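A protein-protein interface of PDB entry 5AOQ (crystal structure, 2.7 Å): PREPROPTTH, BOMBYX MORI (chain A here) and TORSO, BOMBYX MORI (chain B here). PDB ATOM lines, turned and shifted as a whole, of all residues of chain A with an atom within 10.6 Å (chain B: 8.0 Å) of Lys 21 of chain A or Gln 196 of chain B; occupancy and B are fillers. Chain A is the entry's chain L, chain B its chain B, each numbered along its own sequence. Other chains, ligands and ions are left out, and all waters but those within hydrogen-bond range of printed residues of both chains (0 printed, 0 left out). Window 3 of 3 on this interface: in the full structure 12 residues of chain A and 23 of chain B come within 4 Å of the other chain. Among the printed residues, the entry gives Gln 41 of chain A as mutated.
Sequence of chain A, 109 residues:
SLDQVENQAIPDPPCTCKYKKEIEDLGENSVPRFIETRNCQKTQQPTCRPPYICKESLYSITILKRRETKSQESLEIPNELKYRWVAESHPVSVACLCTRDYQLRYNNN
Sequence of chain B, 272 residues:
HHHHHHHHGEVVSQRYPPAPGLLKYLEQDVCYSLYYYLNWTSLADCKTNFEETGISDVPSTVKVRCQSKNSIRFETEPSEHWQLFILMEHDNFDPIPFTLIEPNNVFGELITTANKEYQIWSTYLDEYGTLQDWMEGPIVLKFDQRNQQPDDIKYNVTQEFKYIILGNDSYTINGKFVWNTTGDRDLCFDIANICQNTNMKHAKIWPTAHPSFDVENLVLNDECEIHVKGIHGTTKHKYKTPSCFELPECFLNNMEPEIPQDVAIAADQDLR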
ATOM      1  N   CYS A  17     -17.419  19.301   4.265  1.00  0.00           N
ATOM      2  CA  CYS A  17     -17.186  17.951   4.770  1.00  0.00           C
ATOM      3  C   CYS A  17     -16.238  17.190   3.849  1.00  0.00           C
ATOM      4  O   CYS A  17     -16.452  17.130   2.639  1.00  0.00           O
ATOM      5  CB  CYS A  17     -18.506  17.190   4.897  1.00  0.00           C
ATOM      6  SG  CYS A  17     -19.890  18.194   5.469  1.00  0.00           S
ATOM      7  N   LYS A  18     -15.191  16.611   4.427  1.00  0.00           N
ATOM      8  CA  LYS A  18     -14.240  15.807   3.665  1.00  0.00           C
ATOM      9  C   LYS A  18     -14.885  14.497   3.213  1.00  0.00           C
ATOM     10  O   LYS A  18     -15.502  13.792   4.013  1.00  0.00           O
ATOM     11  CB  LYS A  18     -12.981  15.534   4.493  1.00  0.00           C
ATOM     12  CG  LYS A  18     -13.228  14.915   5.865  1.00  0.00           C
ATOM     13  CD  LYS A  18     -12.214  15.426   6.881  1.00  0.00           C
ATOM     14  CE  LYS A  18     -12.474  14.869   8.272  1.00  0.00           C
ATOM     15  NZ  LYS A  18     -13.804  15.276   8.806  1.00  0.00           N
ATOM     16  N   TYR A  19     -14.732  14.181   1.928  1.00  0.00           N
ATOM     17  CA  TYR A  19     -15.427  13.051   1.313  1.00  0.00           C
ATOM     18  C   TYR A  19     -14.494  11.877   1.010  1.00  0.00           C
ATOM     19  O   TYR A  19     -13.280  12.048   0.891  1.00  0.00           O
ATOM     20  CB  TYR A  19     -16.129  13.509   0.028  1.00  0.00           C
ATOM     21  CG  TYR A  19     -15.202  13.989  -1.066  1.00  0.00           C
ATOM     22  CD1 TYR A  19     -14.676  13.100  -1.994  1.00  0.00           C
ATOM     23  CD2 TYR A  19     -14.867  15.330  -1.183  1.00  0.00           C
ATOM     24  CE1 TYR A  19     -13.836  13.531  -2.999  1.00  0.00           C
ATOM     25  CE2 TYR A  19     -14.026  15.772  -2.187  1.00  0.00           C
ATOM     26  CZ  TYR A  19     -13.514  14.867  -3.092  1.00  0.00           C
ATOM     27  OH  TYR A  19     -12.676  15.299  -4.094  1.00  0.00           O
ATOM     28  N   LYS A  20     -15.082  10.688   0.890  1.00  0.00           N
ATOM     29  CA  LYS A  20     -14.348   9.459   0.588  1.00  0.00           C
ATOM     30  C   LYS A  20     -14.720   8.916  -0.789  1.00  0.00           C
ATOM     31  O   LYS A  20     -15.901   8.829  -1.125  1.00  0.00           O
ATOM     32  CB  LYS A  20     -14.636   8.388   1.643  1.00  0.00           C
ATOM     33  CG  LYS A  20     -13.798   7.122   1.493  1.00  0.00           C
ATOM     34  CD  LYS A  20     -14.329   5.978   2.350  1.00  0.00           C
ATOM     35  CE  LYS A  20     -14.267   6.285   3.835  1.00  0.00           C
ATOM     36  NZ  LYS A  20     -14.763   5.139   4.646  1.00  0.00           N
ATOM     37  N   LYS A  21     -13.715   8.542  -1.577  1.00  0.00           N
ATOM     38  CA  LYS A  21     -13.949   7.969  -2.901  1.00  0.00           C
ATOM     39  C   LYS A  21     -14.099   6.450  -2.820  1.00  0.00           C
ATOM     40  O   LYS A  21     -13.449   5.798  -2.003  1.00  0.00           O
ATOM     41  CB  LYS A  21     -12.814   8.330  -3.861  1.00  0.00           C
ATOM     42  CG  LYS A  21     -12.892   9.746  -4.404  1.00  0.00           C
ATOM     43  CD  LYS A  21     -11.760  10.030  -5.375  1.00  0.00           C
ATOM     44  CE  LYS A  21     -11.819  11.453  -5.906  1.00  0.00           C
ATOM     45  NZ  LYS A  21     -10.754  11.721  -6.913  1.00  0.00           N
ATOM     46  N   GLU A  22     -14.956   5.898  -3.675  1.00  0.00           N
ATOM     47  CA  GLU A  22     -15.196   4.457  -3.721  1.00  0.00           C
ATOM     48  C   GLU A  22     -15.541   4.012  -5.141  1.00  0.00           C
ATOM     49  O   GLU A  22     -15.856   4.842  -5.994  1.00  0.00           O
ATOM     50  CB  GLU A  22     -16.323   4.067  -2.761  1.00  0.00           C
ATOM     51  CG  GLU A  22     -16.028   4.363  -1.298  1.00  0.00           C
ATOM     52  CD  GLU A  22     -17.117   3.868  -0.369  1.00  0.00           C
ATOM     53  OE1 GLU A  22     -18.163   3.402  -0.870  1.00  0.00           O
ATOM     54  OE2 GLU A  22     -16.931   3.946   0.863  1.00  0.00           O
ATOM     55  N   ILE A  23     -15.471   2.705  -5.386  1.00  0.00           N
ATOM     56  CA  ILE A  23     -15.739   2.148  -6.712  1.00  0.00           C
ATOM     57  C   ILE A  23     -16.996   1.282  -6.747  1.00  0.00           C
ATOM     58  O   ILE A  23     -17.240   0.473  -5.850  1.00  0.00           O
ATOM     59  CB  ILE A  23     -14.547   1.304  -7.212  1.00  0.00           C
ATOM     60  CG1 ILE A  23     -13.274   2.153  -7.267  1.00  0.00           C
ATOM     61  CG2 ILE A  23     -14.841   0.700  -8.586  1.00  0.00           C
ATOM     62  CD1 ILE A  23     -13.355   3.342  -8.206  1.00  0.00           C
ATOM     63  N   GLU A  24     -17.785   1.471  -7.803  1.00  0.00           N
ATOM     64  CA  GLU A  24     -18.970   0.658  -8.066  1.00  0.00           C
ATOM     65  C   GLU A  24     -18.726  -0.252  -9.265  1.00  0.00           C
ATOM     66  O   GLU A  24     -18.483   0.230 -10.369  1.00  0.00           O
ATOM     67  CB  GLU A  24     -20.182   1.553  -8.323  1.00  0.00           C
ATOM     68  CG  GLU A  24     -20.946   1.944  -7.070  1.00  0.00           C
ATOM     69  CD  GLU A  24     -21.767   0.800  -6.503  1.00  0.00           C
ATOM     70  OE1 GLU A  24     -21.728  -0.310  -7.074  1.00  0.00           O
ATOM     71  OE2 GLU A  24     -22.457   1.014  -5.484  1.00  0.00           O
ATOM     72  N   ILE A  35     -17.588   2.586 -11.567  1.00  0.00           N
ATOM     73  CA  ILE A  35     -18.084   3.948 -11.350  1.00  0.00           C
ATOM     74  C   ILE A  35     -17.482   4.579 -10.097  1.00  0.00           C
ATOM     75  O   ILE A  35     -17.327   3.922  -9.068  1.00  0.00           O
ATOM     76  CB  ILE A  35     -19.631   3.963 -11.248  1.00  0.00           C
ATOM     77  CG1 ILE A  35     -20.264   4.205 -12.619  1.00  0.00           C
ATOM     78  CG2 ILE A  35     -20.126   5.046 -10.285  1.00  0.00           C
ATOM     79  CD1 ILE A  35     -19.741   3.308 -13.725  1.00  0.00           C
ATOM     80  N   GLU A  36     -17.151   5.864 -10.205  1.00  0.00           N
ATOM     81  CA  GLU A  36     -16.582   6.623  -9.097  1.00  0.00           C
ATOM     82  C   GLU A  36     -17.679   7.181  -8.195  1.00  0.00           C
ATOM     83  O   GLU A  36     -18.559   7.910  -8.656  1.00  0.00           O
ATOM     84  CB  GLU A  36     -15.709   7.765  -9.631  1.00  0.00           C
ATOM     85  CG  GLU A  36     -15.062   8.626  -8.558  1.00  0.00           C
ATOM     86  CD  GLU A  36     -14.173   9.711  -9.142  1.00  0.00           C
ATOM     87  OE1 GLU A  36     -13.828   9.623 -10.338  1.00  0.00           O
ATOM     88  OE2 GLU A  36     -13.826  10.657  -8.403  1.00  0.00           O
ATOM     89  N   THR A  37     -17.616   6.831  -6.913  1.00  0.00           N
ATOM     90  CA  THR A  37     -18.599   7.276  -5.929  1.00  0.00           C
ATOM     91  C   THR A  37     -17.912   8.014  -4.785  1.00  0.00           C
ATOM     92  O   THR A  37     -17.035   7.465  -4.118  1.00  0.00           O
ATOM     93  CB  THR A  37     -19.406   6.093  -5.359  1.00  0.00           C
ATOM     94  OG1 THR A  37     -20.035   5.379  -6.431  1.00  0.00           O
ATOM     95  CG2 THR A  37     -20.472   6.583  -4.384  1.00  0.00           C
ATOM     96  N   ARG A  38     -18.328   9.258  -4.563  1.00  0.00           N
ATOM     97  CA  ARG A  38     -17.745  10.103  -3.528  1.00  0.00           C
ATOM     98  C   ARG A  38     -18.693  10.252  -2.341  1.00  0.00           C
ATOM     99  O   ARG A  38     -19.578  11.108  -2.343  1.00  0.00           O
ATOM    100  CB  ARG A  38     -17.398  11.476  -4.107  1.00  0.00           C
ATOM    101  CG  ARG A  38     -16.410  11.413  -5.260  1.00  0.00           C
ATOM    102  CD  ARG A  38     -16.274  12.750  -5.961  1.00  0.00           C
ATOM    103  NE  ARG A  38     -15.352  12.684  -7.092  1.00  0.00           N
ATOM    104  CZ  ARG A  38     -15.132  13.686  -7.939  1.00  0.00           C
ATOM    105  NH1 ARG A  38     -15.766  14.841  -7.787  1.00  0.00           N
ATOM    106  NH2 ARG A  38     -14.277  13.532  -8.939  1.00  0.00           N
ATOM    107  N   ASN A  39     -18.495   9.416  -1.327  1.00  0.00           N
ATOM    108  CA  ASN A  39     -19.349   9.415  -0.142  1.00  0.00           C
ATOM    109  C   ASN A  39     -18.855  10.392   0.920  1.00  0.00           C
ATOM    110  O   ASN A  39     -17.823  11.033   0.749  1.00  0.00           O
ATOM    111  CB  ASN A  39     -19.430   8.005   0.442  1.00  0.00           C
ATOM    112  CG  ASN A  39     -19.919   6.988  -0.567  1.00  0.00           C
ATOM    113  OD1 ASN A  39     -19.210   6.040  -0.904  1.00  0.00           O
ATOM    114  ND2 ASN A  39     -21.135   7.182  -1.061  1.00  0.00           N
ATOM    115  N   CYS A  40     -19.594  10.493   2.021  1.00  0.00           N
ATOM    116  CA  CYS A  40     -19.339  11.516   3.031  1.00  0.00           C
ATOM    117  C   CYS A  40     -18.269  11.133   4.053  1.00  0.00           C
ATOM    118  O   CYS A  40     -18.036  11.868   5.013  1.00  0.00           O
ATOM    119  CB  CYS A  40     -20.641  11.849   3.761  1.00  0.00           C
ATOM    120  SG  CYS A  40     -21.616  13.136   2.968  1.00  0.00           S
ATOM    121  N   GLN A  41     -17.617   9.994   3.842  1.00  0.00           N
ATOM    122  CA  GLN A  41     -16.581   9.517   4.758  1.00  0.00           C
ATOM    123  C   GLN A  41     -17.122   9.367   6.176  1.00  0.00           C
ATOM    124  O   GLN A  41     -16.810  10.166   7.059  1.00  0.00           O
ATOM    125  CB  GLN A  41     -15.379  10.462   4.746  1.00  0.00           C
ATOM    126  N   SER A  93     -23.616   8.978  -5.036  1.00  0.00           N
ATOM    127  CA  SER A  93     -22.997  10.041  -4.259  1.00  0.00           C
ATOM    128  C   SER A  93     -21.781  10.558  -5.013  1.00  0.00           C
ATOM    129  O   SER A  93     -20.940   9.776  -5.457  1.00  0.00           O
ATOM    130  CB  SER A  93     -22.600   9.542  -2.869  1.00  0.00           C
ATOM    131  OG  SER A  93     -22.058  10.592  -2.085  1.00  0.00           O
ATOM    132  N   VAL A  94     -21.696  11.876  -5.157  1.00  0.00           N
ATOM    133  CA  VAL A  94     -20.635  12.502  -5.938  1.00  0.00           C
ATOM    134  C   VAL A  94     -20.022  13.689  -5.195  1.00  0.00           C
ATOM    135  O   VAL A  94     -19.090  14.331  -5.680  1.00  0.00           O
ATOM    136  CB  VAL A  94     -21.175  12.953  -7.312  1.00  0.00           C
ATOM    137  CG1 VAL A  94     -22.003  14.230  -7.180  1.00  0.00           C
ATOM    138  CG2 VAL A  94     -20.036  13.125  -8.313  1.00  0.00           C
ATOM    139  N   ALA A  95     -20.552  13.976  -4.011  1.00  0.00           N
ATOM    140  CA  ALA A  95     -20.013  15.031  -3.167  1.00  0.00           C
ATOM    141  C   ALA A  95     -20.651  14.943  -1.792  1.00  0.00           C
ATOM    142  O   ALA A  95     -21.699  14.318  -1.628  1.00  0.00           O
ATOM    143  CB  ALA A  95     -20.257  16.400  -3.783  1.00  0.00           C
ATOM    144  N   CYS A  96     -20.013  15.568  -0.809  1.00  0.00           N
ATOM    145  CA  CYS A  96     -20.579  15.663   0.530  1.00  0.00           C
ATOM    146  C   CYS A  96     -20.802  17.124   0.887  1.00  0.00           C
ATOM    147  O   CYS A  96     -19.888  17.815   1.341  1.00  0.00           O
ATOM    148  CB  CYS A  96     -19.673  14.994   1.563  1.00  0.00           C
ATOM    149  SG  CYS A  96     -20.467  14.798   3.176  1.00  0.00           S
ATOM    150  N   ILE B 194      -8.395   4.011  -7.977  1.00  0.00           N
ATOM    151  CA  ILE B 194      -8.815   5.398  -7.806  1.00  0.00           C
ATOM    152  C   ILE B 194      -8.043   6.058  -6.667  1.00  0.00           C
ATOM    153  O   ILE B 194      -7.637   5.392  -5.711  1.00  0.00           O
ATOM    154  CB  ILE B 194     -10.338   5.487  -7.536  1.00  0.00           C
ATOM    155  CG1 ILE B 194     -10.810   6.942  -7.444  1.00  0.00           C
ATOM    156  CG2 ILE B 194     -10.703   4.730  -6.266  1.00  0.00           C
ATOM    157  CD1 ILE B 194     -10.625   7.740  -8.716  1.00  0.00           C
ATOM    158  N   CYS B 195      -7.841   7.368  -6.781  1.00  0.00           N
ATOM    159  CA  CYS B 195      -7.166   8.147  -5.748  1.00  0.00           C
ATOM    160  C   CYS B 195      -7.934   9.422  -5.421  1.00  0.00           C
ATOM    161  O   CYS B 195      -8.773   9.873  -6.199  1.00  0.00           O
ATOM    162  CB  CYS B 195      -5.744   8.502  -6.184  1.00  0.00           C
ATOM    163  SG  CYS B 195      -4.656   7.090  -6.435  1.00  0.00           S
ATOM    164  N   GLN B 196      -7.628  10.000  -4.263  1.00  0.00           N
ATOM    165  CA  GLN B 196      -8.305  11.199  -3.778  1.00  0.00           C
ATOM    166  C   GLN B 196      -8.118  12.388  -4.719  1.00  0.00           C
ATOM    167  O   GLN B 196      -8.955  13.289  -4.755  1.00  0.00           O
ATOM    168  CB  GLN B 196      -7.797  11.551  -2.376  1.00  0.00           C
ATOM    169  CG  GLN B 196      -8.517  12.702  -1.700  1.00  0.00           C
ATOM    170  CD  GLN B 196      -7.940  13.013  -0.332  1.00  0.00           C
ATOM    171  OE1 GLN B 196      -7.167  12.230   0.220  1.00  0.00           O
ATOM    172  NE2 GLN B 196      -8.308  14.164   0.219  1.00  0.00           N
ATOM    173  N   ASN B 197      -7.021  12.387  -5.476  1.00  0.00           N
ATOM    174  CA  ASN B 197      -6.711  13.490  -6.386  1.00  0.00           C
ATOM    175  C   ASN B 197      -6.259  13.005  -7.762  1.00  0.00           C
ATOM    176  O   ASN B 197      -5.431  13.640  -8.416  1.00  0.00           O
ATOM    177  CB  ASN B 197      -5.636  14.390  -5.773  1.00  0.00           C
ATOM    178  CG  ASN B 197      -6.113  15.093  -4.519  1.00  0.00           C
ATOM    179  OD1 ASN B 197      -6.773  16.130  -4.589  1.00  0.00           O
ATOM    180  ND2 ASN B 197      -5.788  14.526  -3.361  1.00  0.00           N
ATOM    181  N   THR B 198      -6.806  11.873  -8.193  1.00  0.00           N
ATOM    182  CA  THR B 198      -6.578  11.377  -9.546  1.00  0.00           C
ATOM    183  C   THR B 198      -7.816  10.649 -10.044  1.00  0.00           C
ATOM    184  O   THR B 198      -8.441   9.891  -9.302  1.00  0.00           O
ATOM    185  CB  THR B 198      -5.366  10.425  -9.617  1.00  0.00           C
ATOM    186  OG1 THR B 198      -4.204  11.085  -9.101  1.00  0.00           O
ATOM    187  CG2 THR B 198      -5.102   9.989 -11.055  1.00  0.00           C
ATOM    188  N   ASN B 199      -8.172  10.887 -11.302  1.00  0.00           N
ATOM    189  CA  ASN B 199      -9.334  10.243 -11.898  1.00  0.00           C
ATOM    190  C   ASN B 199      -9.109   8.742 -12.033  1.00  0.00           C
ATOM    191  O   ASN B 199      -7.975   8.286 -12.184  1.00  0.00           O
ATOM    192  CB  ASN B 199      -9.650  10.861 -13.260  1.00  0.00           C
ATOM    193  CG  ASN B 199     -10.316  12.220 -13.142  1.00  0.00           C
ATOM    194  OD1 ASN B 199     -11.109  12.460 -12.231  1.00  0.00           O
ATOM    195  ND2 ASN B 199      -9.993  13.120 -14.064  1.00  0.00           N
ATOM    196  N   MET B 200     -10.198   7.985 -11.966  1.00  0.00           N
ATOM    197  CA  MET B 200     -10.139   6.527 -11.955  1.00  0.00           C
ATOM    198  C   MET B 200      -9.385   5.965 -13.156  1.00  0.00           C
ATOM    199  O   MET B 200      -9.361   6.569 -14.228  1.00  0.00           O
ATOM    200  CB  MET B 200     -11.550   5.940 -11.938  1.00  0.00           C
ATOM    201  CG  MET B 200     -11.588   4.421 -11.784  1.00  0.00           C
ATOM    202  SD  MET B 200     -13.236   3.692 -11.876  1.00  0.00           S
ATOM    203  CE  MET B 200     -14.261   4.995 -11.211  1.00  0.00           C
ATOM    204  N   LEU B 218      -0.092   9.888 -10.503  1.00  0.00           N
ATOM    205  CA  LEU B 218      -0.231   9.862  -9.052  1.00  0.00           C
ATOM    206  C   LEU B 218       0.453  11.082  -8.447  1.00  0.00           C
ATOM    207  O   LEU B 218       1.247  11.748  -9.113  1.00  0.00           O
ATOM    208  CB  LEU B 218       0.368   8.576  -8.477  1.00  0.00           C
ATOM    209  CG  LEU B 218      -0.339   7.267  -8.834  1.00  0.00           C
ATOM    210  CD1 LEU B 218       0.469   6.081  -8.332  1.00  0.00           C
ATOM    211  CD2 LEU B 218      -1.749   7.232  -8.263  1.00  0.00           C
ATOM    212  N   VAL B 219       0.140  11.373  -7.187  1.00  0.00           N
ATOM    213  CA  VAL B 219       0.754  12.493  -6.477  1.00  0.00           C
ATOM    214  C   VAL B 219       1.196  12.059  -5.083  1.00  0.00           C
ATOM    215  O   VAL B 219       0.843  10.975  -4.617  1.00  0.00           O
ATOM    216  CB  VAL B 219      -0.211  13.697  -6.369  1.00  0.00           C
ATOM    217  CG1 VAL B 219      -0.582  14.209  -7.752  1.00  0.00           C
ATOM    218  CG2 VAL B 219      -1.458  13.326  -5.584  1.00  0.00           C
ATOM    219  N   ASN B 221       1.564  11.759  -1.037  1.00  0.00           N
ATOM    220  CA  ASN B 221       0.692  11.761   0.136  1.00  0.00           C
ATOM    221  C   ASN B 221      -0.785  11.672  -0.231  1.00  0.00           C
ATOM    222  O   ASN B 221      -1.627  12.328   0.383  1.00  0.00           O
ATOM    223  CB  ASN B 221       0.938  13.016   0.976  1.00  0.00           C
ATOM    224  CG  ASN B 221       2.379  13.143   1.425  1.00  0.00           C
ATOM    225  OD1 ASN B 221       2.958  12.200   1.960  1.00  0.00           O
ATOM    226  ND2 ASN B 221       2.968  14.314   1.206  1.00  0.00           N
ATOM    227  N   ASP B 222      -1.093  10.850  -1.229  1.00  0.00           N
ATOM    228  CA  ASP B 222      -2.462  10.688  -1.704  1.00  0.00           C
ATOM    229  C   ASP B 222      -3.058   9.380  -1.201  1.00  0.00           C
ATOM    230  O   ASP B 222      -2.421   8.330  -1.273  1.00  0.00           O
ATOM    231  CB  ASP B 222      -2.493  10.732  -3.233  1.00  0.00           C
ATOM    232  CG  ASP B 222      -3.877  11.013  -3.783  1.00  0.00           C
ATOM    233  OD1 ASP B 222      -4.867  10.680  -3.103  1.00  0.00           O
ATOM    234  OD2 ASP B 222      -3.973  11.574  -4.895  1.00  0.00           O
ATOM    235  N   GLU B 223      -4.288   9.452  -0.699  1.00  0.00           N
ATOM    236  CA  GLU B 223      -4.982   8.277  -0.183  1.00  0.00           C
ATOM    237  C   GLU B 223      -5.727   7.555  -1.301  1.00  0.00           C
ATOM    238  O   GLU B 223      -6.809   7.977  -1.712  1.00  0.00           O
ATOM    239  CB  GLU B 223      -5.954   8.677   0.929  1.00  0.00           C
ATOM    240  CG  GLU B 223      -6.540   7.497   1.694  1.00  0.00           C
ATOM    241  CD  GLU B 223      -5.489   6.715   2.461  1.00  0.00           C
ATOM    242  OE1 GLU B 223      -4.446   7.304   2.818  1.00  0.00           O
ATOM    243  OE2 GLU B 223      -5.708   5.510   2.706  1.00  0.00           O
ATOM    244  N   CYS B 224      -5.136   6.466  -1.784  1.00  0.00           N
ATOM    245  CA  CYS B 224      -5.679   5.720  -2.913  1.00  0.00           C
ATOM    246  C   CYS B 224      -6.341   4.405  -2.506  1.00  0.00           C
ATOM    247  O   CYS B 224      -6.204   3.944  -1.370  1.00  0.00           O
ATOM    248  CB  CYS B 224      -4.571   5.421  -3.918  1.00  0.00           C
ATOM    249  SG  CYS B 224      -3.752   6.862  -4.631  1.00  0.00           S
ATOM    250  N   GLU B 225      -7.041   3.802  -3.465  1.00  0.00           N
ATOM    251  CA  GLU B 225      -7.636   2.484  -3.287  1.00  0.00           C
ATOM    252  C   GLU B 225      -7.703   1.747  -4.624  1.00  0.00           C
ATOM    253  O   GLU B 225      -8.004   2.348  -5.664  1.00  0.00           O
ATOM    254  CB  GLU B 225      -9.033   2.600  -2.673  1.00  0.00           C
ATOM    255  CG  GLU B 225      -9.670   1.262  -2.327  1.00  0.00           C
ATOM    256  CD  GLU B 225     -11.030   1.413  -1.671  1.00  0.00           C
ATOM    257  OE1 GLU B 225     -11.555   2.546  -1.640  1.00  0.00           O
ATOM    258  OE2 GLU B 225     -11.572   0.398  -1.183  1.00  0.00           O
ATOM    259  N   HIS B 227      -9.101  -2.027  -6.419  1.00  0.00           N
ATOM    260  CA  HIS B 227      -9.849  -3.275  -6.366  1.00  0.00           C
ATOM    261  C   HIS B 227      -9.373  -4.239  -7.443  1.00  0.00           C
ATOM    262  O   HIS B 227      -9.269  -3.870  -8.621  1.00  0.00           O
ATOM    263  CB  HIS B 227     -11.344  -3.010  -6.525  1.00  0.00           C
ATOM    264  CG  HIS B 227     -11.847  -1.887  -5.675  1.00  0.00           C
ATOM    265  ND1 HIS B 227     -12.183  -2.048  -4.348  1.00  0.00           N
ATOM    266  CD2 HIS B 227     -12.057  -0.582  -5.960  1.00  0.00           C
ATOM    267  CE1 HIS B 227     -12.587  -0.891  -3.855  1.00  0.00           C
ATOM    268  NE2 HIS B 227     -12.520   0.016  -4.814  1.00  0.00           N
ATOM    269  N   LYS B 238      -6.828  -0.716  -0.015  1.00  0.00           N
ATOM    270  CA  LYS B 238      -6.505   0.685   0.238  1.00  0.00           C
ATOM    271  C   LYS B 238      -4.997   0.859   0.319  1.00  0.00           C
ATOM    272  O   LYS B 238      -4.287  -0.045   0.758  1.00  0.00           O
ATOM    273  CB  LYS B 238      -7.149   1.171   1.537  1.00  0.00           C
ATOM    274  CG  LYS B 238      -8.661   1.261   1.504  1.00  0.00           C
ATOM    275  CD  LYS B 238      -9.197   1.808   2.819  1.00  0.00           C
ATOM    276  CE  LYS B 238     -10.708   1.936   2.801  1.00  0.00           C
ATOM    277  NZ  LYS B 238     -11.234   2.454   4.096  1.00  0.00           N
ATOM    278  N   TYR B 239      -4.505   2.020  -0.099  1.00  0.00           N
ATOM    279  CA  TYR B 239      -3.074   2.286  -0.020  1.00  0.00           C
ATOM    280  C   TYR B 239      -2.782   3.775  -0.161  1.00  0.00           C
ATOM    281  O   TYR B 239      -3.520   4.499  -0.828  1.00  0.00           O
ATOM    282  CB  TYR B 239      -2.321   1.504  -1.096  1.00  0.00           C
ATOM    283  CG  TYR B 239      -2.535   2.023  -2.500  1.00  0.00           C
ATOM    284  CD1 TYR B 239      -3.608   1.597  -3.271  1.00  0.00           C
ATOM    285  CD2 TYR B 239      -1.657   2.939  -3.054  1.00  0.00           C
ATOM    286  CE1 TYR B 239      -3.797   2.077  -4.555  1.00  0.00           C
ATOM    287  CE2 TYR B 239      -1.833   3.421  -4.334  1.00  0.00           C
ATOM    288  CZ  TYR B 239      -2.906   2.986  -5.081  1.00  0.00           C
ATOM    289  OH  TYR B 239      -3.090   3.467  -6.356  1.00  0.00           O
ATOM    290  N   LYS B 240      -1.702   4.221   0.472  1.00  0.00           N
ATOM    291  CA  LYS B 240      -1.302   5.624   0.433  1.00  0.00           C
ATOM    292  C   LYS B 240      -0.006   5.793  -0.348  1.00  0.00           C
ATOM    293  O   LYS B 240       0.945   5.035  -0.161  1.00  0.00           O
ATOM    294  CB  LYS B 240      -1.127   6.173   1.850  1.00  0.00           C
ATOM    295  CG  LYS B 240      -0.877   7.673   1.903  1.00  0.00           C
ATOM    296  CD  LYS B 240      -0.695   8.160   3.332  1.00  0.00           C
ATOM    297  CE  LYS B 240      -0.489   9.667   3.389  1.00  0.00           C
ATOM    298  NZ  LYS B 240      -1.668  10.422   2.878  1.00  0.00           N
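O of Gln 196 of chain B is in hydrogen-bond range of NZ of Lys 21 of chain A, at 3.2 Å. NZ of Lys 21 of chain A is in hydrogen-bond range of O of Cys 195 of chain B (2.8 Å).
The side-chain carboxylate of Asp 222 of chain B is in hydrogen-bond range of the backbone NH of Gln 196 of chain B (3.1 Å). The backbone NH of Glu 225 of chain B is in hydrogen-bond range of the backbone carbonyl oxygen of Ile 194 of chain B (2.8 Å). The side-chain carboxylate of Glu 36 of chain A is in salt-bridge range of the guanidinium group of Arg 38 of chain A. SG of Cys 40 of chain A forms a disulfide with SG of Cys 96 of chain A, at 2.0 Å. The side-chain sulfur (SG) of Cys 195 of chain B forms a disulfide with the side-chain sulfur (SG) of Cys 224 of chain B, at 2.0 Å. The backbone carbonyl oxygen (O) of Glu 24 of chain A is in hydrogen-bond range of the backbone NH (N) of Ile 35 of chain A, 2.8 Å away.
Lys 21 of chain A touches Ile 194 of chain B. Thr 198 of chain B touches Lys 21 of chain A (O to NZ, 3.8 Å). O of Lys 21 of chain A touches OE1 of Glu 225 of chain B, 3.8 Å away. Ile 194 of chain B touches Ile 23 of chain A. Ile 23 of chain A touches Met 200 of chain B. CD2 of His 227 of chain B touches CG1 of Ile 23 of chain A, at 3.3 Å. Met 200 of chain B touches Ile 35 of chain A. Glu 36 of chain A touches Met 200 of chain B (N to CE, 3.2 Å).
Lys 21 of chain A touches just these residues of chain B: Ile 194, Cys 195, Gln 196, Thr 198 and Glu 225. Printed residues of chain A within 4 Å of Gln 196 of chain B: Lys 21 (3.2 Å). No residue of chain A comes within 4 Å of Asp 222 of chain B. Of the printed residues of chain A, His 227 of chain B touches Ile 23 (3.3 Å). Printed residues of chain A within 4 Å of Met 200 of chain B: Ile 23, Ile 35 and Glu 36. Of the printed residues of chain B, Ile 35 of chain A touches Met 200 (3.4 Å). Cys 17 of chain A touches none of the printed residues of chain B. Cys 40 of chain A touches none of the printed residues of chain B. The nearest residue of chain B that does not touch Lys 21 of chain A is Asn 197 of chain B (4.1 Å). The nearest residue of chain A that does not touch Gln 196 of chain B is Tyr 19 of chain A (4.3 Å). The nearest printed residue of chain B that does not touch Glu 36 of chain A is Ile 194 of chain B (4.1 Å).
Of the 18 printed residues of chain B, 7 touch a printed residue of chain A. Hydrophobic or aromatic side chains of chain B within 4 Å of the printed part of chain A: Ile 194, Met 200 and His 227. Printed residues of chain A that touch a printed residue of chain B: Lys 21, Ile 23, Ile 35 and Glu 36. Among the printed residues, no Asp or Glu carboxylate lies within 4 Å of a Lys or Arg side-chain nitrogen of the other chain.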
